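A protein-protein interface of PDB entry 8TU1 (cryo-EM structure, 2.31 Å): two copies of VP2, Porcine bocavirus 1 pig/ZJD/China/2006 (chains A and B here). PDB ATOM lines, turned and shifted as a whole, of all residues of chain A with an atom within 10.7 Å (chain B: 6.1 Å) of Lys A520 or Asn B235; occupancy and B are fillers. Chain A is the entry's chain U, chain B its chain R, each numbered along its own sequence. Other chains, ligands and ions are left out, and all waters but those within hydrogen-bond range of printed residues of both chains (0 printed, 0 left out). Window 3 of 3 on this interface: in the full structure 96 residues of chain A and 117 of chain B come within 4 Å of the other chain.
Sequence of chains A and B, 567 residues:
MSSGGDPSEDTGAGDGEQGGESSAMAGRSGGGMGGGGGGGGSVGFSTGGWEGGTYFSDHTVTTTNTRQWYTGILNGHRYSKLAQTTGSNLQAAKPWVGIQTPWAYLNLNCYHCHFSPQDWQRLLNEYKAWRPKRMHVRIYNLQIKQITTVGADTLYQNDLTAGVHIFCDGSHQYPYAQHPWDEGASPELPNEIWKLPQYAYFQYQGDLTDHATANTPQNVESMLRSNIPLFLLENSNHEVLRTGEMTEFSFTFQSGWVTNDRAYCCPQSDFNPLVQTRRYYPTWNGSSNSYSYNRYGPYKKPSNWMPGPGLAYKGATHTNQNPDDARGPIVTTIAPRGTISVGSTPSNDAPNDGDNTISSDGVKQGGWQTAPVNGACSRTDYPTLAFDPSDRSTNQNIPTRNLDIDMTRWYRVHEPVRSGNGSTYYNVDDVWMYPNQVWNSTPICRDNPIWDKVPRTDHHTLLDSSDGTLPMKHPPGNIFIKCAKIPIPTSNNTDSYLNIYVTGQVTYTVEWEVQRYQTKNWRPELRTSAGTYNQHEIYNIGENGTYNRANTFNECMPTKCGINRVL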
ATOM      1  N   LYS A 128     -11.848 -13.337  -9.699  1.00  0.00           N
ATOM      2  CA  LYS A 128     -12.881 -12.575  -9.009  1.00  0.00           C
ATOM      3  C   LYS A 128     -12.321 -11.315  -8.359  1.00  0.00           C
ATOM      4  O   LYS A 128     -13.065 -10.369  -8.100  1.00  0.00           O
ATOM      5  CB  LYS A 128     -13.582 -13.442  -7.968  1.00  0.00           C
ATOM      6  CG  LYS A 128     -12.707 -13.909  -6.847  1.00  0.00           C
ATOM      7  CD  LYS A 128     -13.512 -14.715  -5.868  1.00  0.00           C
ATOM      8  CE  LYS A 128     -12.662 -15.207  -4.733  1.00  0.00           C
ATOM      9  NZ  LYS A 128     -13.461 -16.000  -3.781  1.00  0.00           N
ATOM     10  N   TYR A 264     -25.998 -11.503  -7.610  1.00  0.00           N
ATOM     11  CA  TYR A 264     -27.192 -11.742  -8.401  1.00  0.00           C
ATOM     12  C   TYR A 264     -28.467 -11.446  -7.631  1.00  0.00           C
ATOM     13  O   TYR A 264     -29.541 -11.416  -8.231  1.00  0.00           O
ATOM     14  CB  TYR A 264     -27.228 -13.191  -8.888  1.00  0.00           C
ATOM     15  CG  TYR A 264     -27.351 -14.193  -7.774  1.00  0.00           C
ATOM     16  CD1 TYR A 264     -28.592 -14.599  -7.321  1.00  0.00           C
ATOM     17  CD2 TYR A 264     -26.231 -14.726  -7.172  1.00  0.00           C
ATOM     18  CE1 TYR A 264     -28.710 -15.496  -6.310  1.00  0.00           C
ATOM     19  CE2 TYR A 264     -26.343 -15.630  -6.156  1.00  0.00           C
ATOM     20  CZ  TYR A 264     -27.585 -16.012  -5.730  1.00  0.00           C
ATOM     21  OH  TYR A 264     -27.703 -16.916  -4.717  1.00  0.00           O
ATOM     22  N   TYR A 517     -11.876 -17.304  -9.195  1.00  0.00           N
ATOM     23  CA  TYR A 517     -13.205 -17.565  -8.672  1.00  0.00           C
ATOM     24  C   TYR A 517     -13.423 -19.066  -8.572  1.00  0.00           C
ATOM     25  O   TYR A 517     -12.822 -19.843  -9.313  1.00  0.00           O
ATOM     26  CB  TYR A 517     -14.281 -16.943  -9.559  1.00  0.00           C
ATOM     27  CG  TYR A 517     -14.425 -17.589 -10.915  1.00  0.00           C
ATOM     28  CD1 TYR A 517     -15.318 -18.626 -11.114  1.00  0.00           C
ATOM     29  CD2 TYR A 517     -13.659 -17.173 -11.989  1.00  0.00           C
ATOM     30  CE1 TYR A 517     -15.451 -19.219 -12.334  1.00  0.00           C
ATOM     31  CE2 TYR A 517     -13.787 -17.759 -13.212  1.00  0.00           C
ATOM     32  CZ  TYR A 517     -14.685 -18.782 -13.383  1.00  0.00           C
ATOM     33  OH  TYR A 517     -14.822 -19.374 -14.605  1.00  0.00           O
ATOM     34  N   GLN A 518     -14.281 -19.464  -7.646  1.00  0.00           N
ATOM     35  CA  GLN A 518     -14.770 -20.829  -7.550  1.00  0.00           C
ATOM     36  C   GLN A 518     -16.266 -20.743  -7.331  1.00  0.00           C
ATOM     37  O   GLN A 518     -16.727 -19.919  -6.539  1.00  0.00           O
ATOM     38  CB  GLN A 518     -14.110 -21.593  -6.403  1.00  0.00           C
ATOM     39  CG  GLN A 518     -12.611 -21.751  -6.526  1.00  0.00           C
ATOM     40  CD  GLN A 518     -12.195 -22.443  -7.804  1.00  0.00           C
ATOM     41  OE1 GLN A 518     -12.858 -23.367  -8.267  1.00  0.00           O
ATOM     42  NE2 GLN A 518     -11.084 -22.006  -8.376  1.00  0.00           N
ATOM     43  N   THR A 519     -17.027 -21.574  -8.025  1.00  0.00           N
ATOM     44  CA  THR A 519     -18.470 -21.496  -7.918  1.00  0.00           C
ATOM     45  C   THR A 519     -19.075 -22.882  -8.022  1.00  0.00           C
ATOM     46  O   THR A 519     -18.532 -23.772  -8.678  1.00  0.00           O
ATOM     47  CB  THR A 519     -19.066 -20.576  -8.997  1.00  0.00           C
ATOM     48  OG1 THR A 519     -20.459 -20.375  -8.744  1.00  0.00           O
ATOM     49  CG2 THR A 519     -18.884 -21.166 -10.380  1.00  0.00           C
ATOM     50  N   LYS A 520     -20.192 -23.064  -7.339  1.00  0.00           N
ATOM     51  CA  LYS A 520     -21.029 -24.231  -7.536  1.00  0.00           C
ATOM     52  C   LYS A 520     -22.166 -23.957  -8.497  1.00  0.00           C
ATOM     53  O   LYS A 520     -23.012 -24.827  -8.688  1.00  0.00           O
ATOM     54  CB  LYS A 520     -21.581 -24.730  -6.203  1.00  0.00           C
ATOM     55  CG  LYS A 520     -20.519 -25.029  -5.185  1.00  0.00           C
ATOM     56  CD  LYS A 520     -19.490 -26.018  -5.668  1.00  0.00           C
ATOM     57  CE  LYS A 520     -20.020 -27.420  -5.677  1.00  0.00           C
ATOM     58  NZ  LYS A 520     -18.946 -28.394  -5.982  1.00  0.00           N
ATOM     59  N   ASN A 521     -22.219 -22.763  -9.076  1.00  0.00           N
ATOM     60  CA  ASN A 521     -23.235 -22.443 -10.066  1.00  0.00           C
ATOM     61  C   ASN A 521     -23.251 -23.508 -11.146  1.00  0.00           C
ATOM     62  O   ASN A 521     -22.214 -23.880 -11.686  1.00  0.00           O
ATOM     63  CB  ASN A 521     -22.949 -21.082 -10.693  1.00  0.00           C
ATOM     64  CG  ASN A 521     -24.052 -20.610 -11.617  1.00  0.00           C
ATOM     65  OD1 ASN A 521     -24.920 -21.370 -12.028  1.00  0.00           O
ATOM     66  ND2 ASN A 521     -23.985 -19.356 -11.992  1.00  0.00           N
ATOM     67  N   TRP A 522     -24.440 -24.007 -11.444  1.00  0.00           N
ATOM     68  CA  TRP A 522     -24.572 -25.010 -12.480  1.00  0.00           C
ATOM     69  C   TRP A 522     -24.494 -24.383 -13.862  1.00  0.00           C
ATOM     70  O   TRP A 522     -23.978 -24.998 -14.797  1.00  0.00           O
ATOM     71  CB  TRP A 522     -25.896 -25.745 -12.311  1.00  0.00           C
ATOM     72  CG  TRP A 522     -26.099 -26.797 -13.303  1.00  0.00           C
ATOM     73  CD1 TRP A 522     -26.877 -26.736 -14.407  1.00  0.00           C
ATOM     74  CD2 TRP A 522     -25.515 -28.092 -13.293  1.00  0.00           C
ATOM     75  NE1 TRP A 522     -26.816 -27.910 -15.089  1.00  0.00           N
ATOM     76  CE2 TRP A 522     -25.985 -28.766 -14.424  1.00  0.00           C
ATOM     77  CE3 TRP A 522     -24.640 -28.751 -12.430  1.00  0.00           C
ATOM     78  CZ2 TRP A 522     -25.610 -30.063 -14.721  1.00  0.00           C
ATOM     79  CZ3 TRP A 522     -24.271 -30.037 -12.726  1.00  0.00           C
ATOM     80  CH2 TRP A 522     -24.751 -30.681 -13.863  1.00  0.00           C
ATOM     81  N   ARG A 523     -24.987 -23.158 -13.996  1.00  0.00           N
ATOM     82  CA  ARG A 523     -25.185 -22.579 -15.305  1.00  0.00           C
ATOM     83  C   ARG A 523     -23.931 -21.867 -15.791  1.00  0.00           C
ATOM     84  O   ARG A 523     -23.101 -21.433 -14.993  1.00  0.00           O
ATOM     85  CB  ARG A 523     -26.345 -21.594 -15.300  1.00  0.00           C
ATOM     86  CG  ARG A 523     -27.683 -22.183 -14.964  1.00  0.00           C
ATOM     87  CD  ARG A 523     -28.757 -21.150 -15.132  1.00  0.00           C
ATOM     88  NE  ARG A 523     -28.870 -20.808 -16.543  1.00  0.00           N
ATOM     89  CZ  ARG A 523     -28.514 -19.642 -17.068  1.00  0.00           C
ATOM     90  NH1 ARG A 523     -28.640 -19.447 -18.368  1.00  0.00           N
ATOM     91  NH2 ARG A 523     -28.044 -18.671 -16.303  1.00  0.00           N
ATOM     92  N   PRO A 524     -23.779 -21.729 -17.101  1.00  0.00           N
ATOM     93  CA  PRO A 524     -22.766 -20.826 -17.631  1.00  0.00           C
ATOM     94  C   PRO A 524     -23.106 -19.385 -17.304  1.00  0.00           C
ATOM     95  O   PRO A 524     -24.256 -19.031 -17.049  1.00  0.00           O
ATOM     96  CB  PRO A 524     -22.818 -21.085 -19.138  1.00  0.00           C
ATOM     97  CG  PRO A 524     -24.190 -21.515 -19.374  1.00  0.00           C
ATOM     98  CD  PRO A 524     -24.601 -22.302 -18.173  1.00  0.00           C
ATOM     99  N   GLU A 525     -22.091 -18.544 -17.337  1.00  0.00           N
ATOM    100  CA  GLU A 525     -22.218 -17.167 -16.907  1.00  0.00           C
ATOM    101  C   GLU A 525     -21.816 -16.220 -18.024  1.00  0.00           C
ATOM    102  O   GLU A 525     -21.223 -16.617 -19.027  1.00  0.00           O
ATOM    103  CB  GLU A 525     -21.372 -16.901 -15.659  1.00  0.00           C
ATOM    104  CG  GLU A 525     -21.860 -17.629 -14.425  1.00  0.00           C
ATOM    105  CD  GLU A 525     -20.974 -17.421 -13.211  1.00  0.00           C
ATOM    106  OE1 GLU A 525     -19.866 -16.873 -13.362  1.00  0.00           O
ATOM    107  OE2 GLU A 525     -21.387 -17.801 -12.097  1.00  0.00           O
ATOM    108  N   ARG A 527     -19.503 -13.686 -19.723  1.00  0.00           N
ATOM    109  CA  ARG A 527     -18.071 -13.464 -19.750  1.00  0.00           C
ATOM    110  C   ARG A 527     -17.768 -12.322 -20.697  1.00  0.00           C
ATOM    111  O   ARG A 527     -18.537 -12.027 -21.611  1.00  0.00           O
ATOM    112  CB  ARG A 527     -17.304 -14.720 -20.159  1.00  0.00           C
ATOM    113  CG  ARG A 527     -17.405 -15.842 -19.164  1.00  0.00           C
ATOM    114  CD  ARG A 527     -16.563 -15.526 -17.950  1.00  0.00           C
ATOM    115  NE  ARG A 527     -16.605 -16.592 -16.961  1.00  0.00           N
ATOM    116  CZ  ARG A 527     -17.451 -16.630 -15.941  1.00  0.00           C
ATOM    117  NH1 ARG A 527     -18.322 -15.648 -15.765  1.00  0.00           N
ATOM    118  NH2 ARG A 527     -17.423 -17.643 -15.093  1.00  0.00           N
ATOM    119  N   ILE A 563     -19.202 -12.736 -13.061  1.00  0.00           N
ATOM    120  CA  ILE A 563     -19.076 -13.798 -12.074  1.00  0.00           C
ATOM    121  C   ILE A 563     -20.082 -13.582 -10.956  1.00  0.00           C
ATOM    122  O   ILE A 563     -20.156 -12.501 -10.366  1.00  0.00           O
ATOM    123  CB  ILE A 563     -17.645 -13.850 -11.524  1.00  0.00           C
ATOM    124  CG1 ILE A 563     -16.657 -14.191 -12.633  1.00  0.00           C
ATOM    125  CG2 ILE A 563     -17.546 -14.890 -10.430  1.00  0.00           C
ATOM    126  CD1 ILE A 563     -15.219 -13.977 -12.235  1.00  0.00           C
ATOM    127  N   ASN A 564     -20.858 -14.611 -10.664  1.00  0.00           N
ATOM    128  CA  ASN A 564     -21.807 -14.567  -9.568  1.00  0.00           C
ATOM    129  C   ASN A 564     -21.116 -14.923  -8.264  1.00  0.00           C
ATOM    130  O   ASN A 564     -20.365 -15.894  -8.193  1.00  0.00           O
ATOM    131  CB  ASN A 564     -22.965 -15.528  -9.830  1.00  0.00           C
ATOM    132  CG  ASN A 564     -23.891 -15.031 -10.909  1.00  0.00           C
ATOM    133  OD1 ASN A 564     -24.016 -13.831 -11.121  1.00  0.00           O
ATOM    134  ND2 ASN A 564     -24.515 -15.952 -11.627  1.00  0.00           N
ATOM    135  N   ARG A 565     -21.362 -14.123  -7.234  1.00  0.00           N
ATOM    136  CA  ARG A 565     -20.943 -14.470  -5.888  1.00  0.00           C
ATOM    137  C   ARG A 565     -22.182 -14.897  -5.119  1.00  0.00           C
ATOM    138  O   ARG A 565     -23.276 -14.387  -5.364  1.00  0.00           O
ATOM    139  CB  ARG A 565     -20.261 -13.309  -5.160  1.00  0.00           C
ATOM    140  CG  ARG A 565     -21.233 -12.279  -4.677  1.00  0.00           C
ATOM    141  CD  ARG A 565     -20.634 -11.260  -3.738  1.00  0.00           C
ATOM    142  NE  ARG A 565     -19.705 -10.351  -4.389  1.00  0.00           N
ATOM    143  CZ  ARG A 565     -18.880  -9.548  -3.735  1.00  0.00           C
ATOM    144  NH1 ARG A 565     -18.084  -8.742  -4.399  1.00  0.00           N
ATOM    145  NH2 ARG A 565     -18.877  -9.529  -2.415  1.00  0.00           N
ATOM    146  N   VAL A 566     -22.010 -15.848  -4.213  1.00  0.00           N
ATOM    147  CA  VAL A 566     -23.075 -16.177  -3.284  1.00  0.00           C
ATOM    148  C   VAL A 566     -22.990 -15.236  -2.094  1.00  0.00           C
ATOM    149  O   VAL A 566     -21.912 -15.023  -1.527  1.00  0.00           O
ATOM    150  CB  VAL A 566     -22.966 -17.649  -2.861  1.00  0.00           C
ATOM    151  CG1 VAL A 566     -24.009 -17.990  -1.821  1.00  0.00           C
ATOM    152  CG2 VAL A 566     -23.114 -18.531  -4.069  1.00  0.00           C
ATOM    153  N   GLN B 173     -20.966 -22.108  -0.161  1.00  0.00           N
ATOM    154  CA  GLN B 173     -21.023 -22.216  -1.608  1.00  0.00           C
ATOM    155  C   GLN B 173     -22.448 -22.060  -2.107  1.00  0.00           C
ATOM    156  O   GLN B 173     -22.679 -21.519  -3.190  1.00  0.00           O
ATOM    157  CB  GLN B 173     -20.453 -23.561  -2.037  1.00  0.00           C
ATOM    158  CG  GLN B 173     -18.989 -23.735  -1.709  1.00  0.00           C
ATOM    159  CD  GLN B 173     -18.120 -22.693  -2.366  1.00  0.00           C
ATOM    160  OE1 GLN B 173     -18.320 -22.340  -3.528  1.00  0.00           O
ATOM    161  NE2 GLN B 173     -17.161 -22.170  -1.617  1.00  0.00           N
ATOM    162  N   TYR B 174     -23.380 -22.575  -1.389  1.00  0.00           N
ATOM    163  CA  TYR B 174     -24.773 -22.473  -1.750  1.00  0.00           C
ATOM    164  C   TYR B 174     -25.437 -21.286  -1.079  1.00  0.00           C
ATOM    165  O   TYR B 174     -24.941 -20.767  -0.078  1.00  0.00           O
ATOM    166  CB  TYR B 174     -25.479 -23.777  -1.414  1.00  0.00           C
ATOM    167  CG  TYR B 174     -24.882 -24.880  -2.229  1.00  0.00           C
ATOM    168  CD1 TYR B 174     -25.303 -25.110  -3.524  1.00  0.00           C
ATOM    169  CD2 TYR B 174     -23.865 -25.665  -1.722  1.00  0.00           C
ATOM    170  CE1 TYR B 174     -24.751 -26.099  -4.278  1.00  0.00           C
ATOM    171  CE2 TYR B 174     -23.309 -26.658  -2.472  1.00  0.00           C
ATOM    172  CZ  TYR B 174     -23.756 -26.875  -3.747  1.00  0.00           C
ATOM    173  OH  TYR B 174     -23.204 -27.869  -4.504  1.00  0.00           O
ATOM    174  N   LEU B 230     -27.838 -21.240 -10.966  1.00  0.00           N
ATOM    175  CA  LEU B 230     -28.599 -22.407 -10.547  1.00  0.00           C
ATOM    176  C   LEU B 230     -27.726 -23.207  -9.601  1.00  0.00           C
ATOM    177  O   LEU B 230     -26.560 -23.469  -9.903  1.00  0.00           O
ATOM    178  CB  LEU B 230     -29.025 -23.272 -11.734  1.00  0.00           C
ATOM    179  CG  LEU B 230     -29.763 -24.559 -11.357  1.00  0.00           C
ATOM    180  CD1 LEU B 230     -31.071 -24.252 -10.664  1.00  0.00           C
ATOM    181  CD2 LEU B 230     -29.991 -25.430 -12.570  1.00  0.00           C
ATOM    182  N   PHE B 231     -28.272 -23.585  -8.457  1.00  0.00           N
ATOM    183  CA  PHE B 231     -27.507 -24.327  -7.468  1.00  0.00           C
ATOM    184  C   PHE B 231     -28.153 -25.679  -7.240  1.00  0.00           C
ATOM    185  O   PHE B 231     -29.313 -25.762  -6.832  1.00  0.00           O
ATOM    186  CB  PHE B 231     -27.383 -23.549  -6.165  1.00  0.00           C
ATOM    187  CG  PHE B 231     -26.634 -22.276  -6.312  1.00  0.00           C
ATOM    188  CD1 PHE B 231     -25.256 -22.278  -6.358  1.00  0.00           C
ATOM    189  CD2 PHE B 231     -27.301 -21.075  -6.405  1.00  0.00           C
ATOM    190  CE1 PHE B 231     -24.562 -21.107  -6.498  1.00  0.00           C
ATOM    191  CE2 PHE B 231     -26.611 -19.905  -6.529  1.00  0.00           C
ATOM    192  CZ  PHE B 231     -25.241 -19.919  -6.579  1.00  0.00           C
ATOM    193  N   LEU B 232     -27.402 -26.728  -7.521  1.00  0.00           N
ATOM    194  CA  LEU B 232     -27.829 -28.099  -7.310  1.00  0.00           C
ATOM    195  C   LEU B 232     -26.901 -28.675  -6.262  1.00  0.00           C
ATOM    196  O   LEU B 232     -25.687 -28.697  -6.458  1.00  0.00           O
ATOM    197  CB  LEU B 232     -27.741 -28.892  -8.608  1.00  0.00           C
ATOM    198  CG  LEU B 232     -28.587 -28.348  -9.748  1.00  0.00           C
ATOM    199  CD1 LEU B 232     -28.283 -29.105 -11.022  1.00  0.00           C
ATOM    200  CD2 LEU B 232     -30.057 -28.407  -9.401  1.00  0.00           C
ATOM    201  N   LEU B 233     -27.460 -29.126  -5.150  1.00  0.00           N
ATOM    202  CA  LEU B 233     -26.611 -29.589  -4.063  1.00  0.00           C
ATOM    203  C   LEU B 233     -25.869 -30.868  -4.409  1.00  0.00           C
ATOM    204  O   LEU B 233     -24.922 -31.228  -3.707  1.00  0.00           O
ATOM    205  CB  LEU B 233     -27.443 -29.771  -2.800  1.00  0.00           C
ATOM    206  CG  LEU B 233     -27.563 -28.525  -1.926  1.00  0.00           C
ATOM    207  CD1 LEU B 233     -28.247 -27.392  -2.652  1.00  0.00           C
ATOM    208  CD2 LEU B 233     -28.328 -28.870  -0.670  1.00  0.00           C
ATOM    209  N   GLU B 234     -26.243 -31.540  -5.492  1.00  0.00           N
ATOM    210  CA  GLU B 234     -25.631 -32.816  -5.822  1.00  0.00           C
ATOM    211  C   GLU B 234     -24.328 -32.690  -6.591  1.00  0.00           C
ATOM    212  O   GLU B 234     -23.715 -33.718  -6.877  1.00  0.00           O
ATOM    213  CB  GLU B 234     -26.622 -33.676  -6.600  1.00  0.00           C
ATOM    214  CG  GLU B 234     -27.773 -34.156  -5.755  1.00  0.00           C
ATOM    215  CD  GLU B 234     -28.851 -33.112  -5.558  1.00  0.00           C
ATOM    216  OE1 GLU B 234     -28.694 -31.979  -6.051  1.00  0.00           O
ATOM    217  OE2 GLU B 234     -29.852 -33.425  -4.889  1.00  0.00           O
ATOM    218  N   ASN B 235     -23.876 -31.486  -6.927  1.00  0.00           N
ATOM    219  CA  ASN B 235     -22.544 -31.335  -7.491  1.00  0.00           C
ATOM    220  C   ASN B 235     -21.495 -31.088  -6.418  1.00  0.00           C
ATOM    221  O   ASN B 235     -20.383 -30.679  -6.739  1.00  0.00           O
ATOM    222  CB  ASN B 235     -22.484 -30.243  -8.565  1.00  0.00           C
ATOM    223  CG  ASN B 235     -22.628 -28.850  -8.014  1.00  0.00           C
ATOM    224  OD1 ASN B 235     -23.058 -28.646  -6.885  1.00  0.00           O
ATOM    225  ND2 ASN B 235     -22.221 -27.876  -8.806  1.00  0.00           N
ATOM    226  N   SER B 236     -21.855 -31.214  -5.151  1.00  0.00           N
ATOM    227  CA  SER B 236     -20.885 -31.120  -4.075  1.00  0.00           C
ATOM    228  C   SER B 236     -20.754 -32.472  -3.384  1.00  0.00           C
ATOM    229  O   SER B 236     -21.457 -33.429  -3.706  1.00  0.00           O
ATOM    230  CB  SER B 236     -21.289 -30.024  -3.080  1.00  0.00           C
ATOM    231  OG  SER B 236     -20.365 -29.930  -2.020  1.00  0.00           O
ATOM    232  N   ASN B 237     -19.849 -32.545  -2.418  1.00  0.00           N
ATOM    233  CA  ASN B 237     -19.593 -33.770  -1.673  1.00  0.00           C
ATOM    234  C   ASN B 237     -20.449 -33.791  -0.420  1.00  0.00           C
ATOM    235  O   ASN B 237     -20.469 -32.818   0.335  1.00  0.00           O
ATOM    236  CB  ASN B 237     -18.124 -33.878  -1.269  1.00  0.00           C
ATOM    237  CG  ASN B 237     -17.216 -34.142  -2.431  1.00  0.00           C
ATOM    238  OD1 ASN B 237     -17.631 -34.671  -3.447  1.00  0.00           O
ATOM    239  ND2 ASN B 237     -15.962 -33.762  -2.289  1.00  0.00           N
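Thr A519 touches none of the printed residues of chain B. Printed residues of chain B within 4 Å of Lys A520: Gln B173, Tyr B174, Leu B230, Asn B235 and Ser B236. Of the printed residues of chain B, Trp A522 touches Leu B230 (2.7 Å) and Leu B232 (3.7 Å). Printed residues of chain A within 4 Å of Leu B230: Lys A520 (3.99 Å), Asn A521 (3.1 Å), Trp A522 (2.7 Å) and Arg A523 (3.7 Å). Of chain A, only Tyr A264, Asn A521 and Val A566 come within 4 Å of Phe B231. Asn B235 touches just one residue of chain A: Lys A520 (2.8 Å). Ser B236 touches just one residue of chain A: Lys A520. The nearest residue of chain A that does not touch Asn B235 is Trp A522 (4.4 Å). The nearest printed residue of chain B that does not touch Trp A522 is Asn B235 (4.4 Å).
N of Asn A521 lies within hydrogen-bond range of OG1 of Thr A519. The side-chain amide nitrogen (ND2) of Asn A521 sits at hydrogen-bond distance from the side-chain carboxylate (OE2) of Glu A525, at 3.0 Å. OD1 of Asn A521 lies within hydrogen-bond range of N of Arg A523, 2.7 Å away. The side-chain amide oxygen of Asn B235 lies within hydrogen-bond range of the side-chain hydroxyl of Tyr B174, 2.5 Å away. ND2 of Asn A564 lies close to ND2 of Asn A521 (3.5 Å). The backbone carbonyl oxygen of Leu B232 lies close to the side-chain amide oxygen of Asn B235.
CG of Lys A520 touches CB of Gln B173, 3.5 Å away. Tyr B174 touches Lys A520. Lys A520 touches Leu B230 (O to O, 3.99 Å). Lys A520 touches Ser B236. Asn A521 touches Phe B231. Trp A522 touches Leu B232 (CD2 to CD1, 3.7 Å). Leu B230 touches Arg A523. Gln B173 touches Val A566 (O to CG2, 3.1 Å). CG1 of Val A566 touches O of Tyr B174 (3.4 Å). Phe B231 touches Val A566.
Of the 16 printed residues of chain A, 6 touch a printed residue of chain B. Hydrophobic or aromatic side chains of chain A that line the printed part of chain B: Tyr A264, Trp A522 and Val A566. Of the 10 printed residues of chain B, 7 touch a printed residue of chain A. Printed residues of chain B that touch a printed residue of chain A: Gln B173, Tyr B174, Leu B230, Phe B231, Leu B232, Asn B235 and Ser B236. Hydrophobic or aromatic side chains of chain B that line the printed part of chain A: Tyr B174, Leu B230, Phe B231 and Leu B232. Along chain B the printed residues that touch a printed residue of chain A span positions 173 to 236. Among the printed residues, 14 pairs touch across the chains. Among the printed residues, no Asp or Glu carboxylate lies within 4 Å of a Lys or Arg side-chain nitrogen of the other chain.
OD1 of Asn A521 sits at hydrogen-bond distance from N of Leu B230 (3.1 Å). NZ of Lys A520 sits at hydrogen-bond distance from O of Asn B235, at 2.8 Å. The backbone carbonyl oxygen (O) of Leu B230 is in hydrogen-bond range of the backbone NH (N) of Trp A522.
No position is printed for both chains. Of the 14 pairs that touch across the chains among the printed residues, none has its exchanged pair printed and touching as well.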
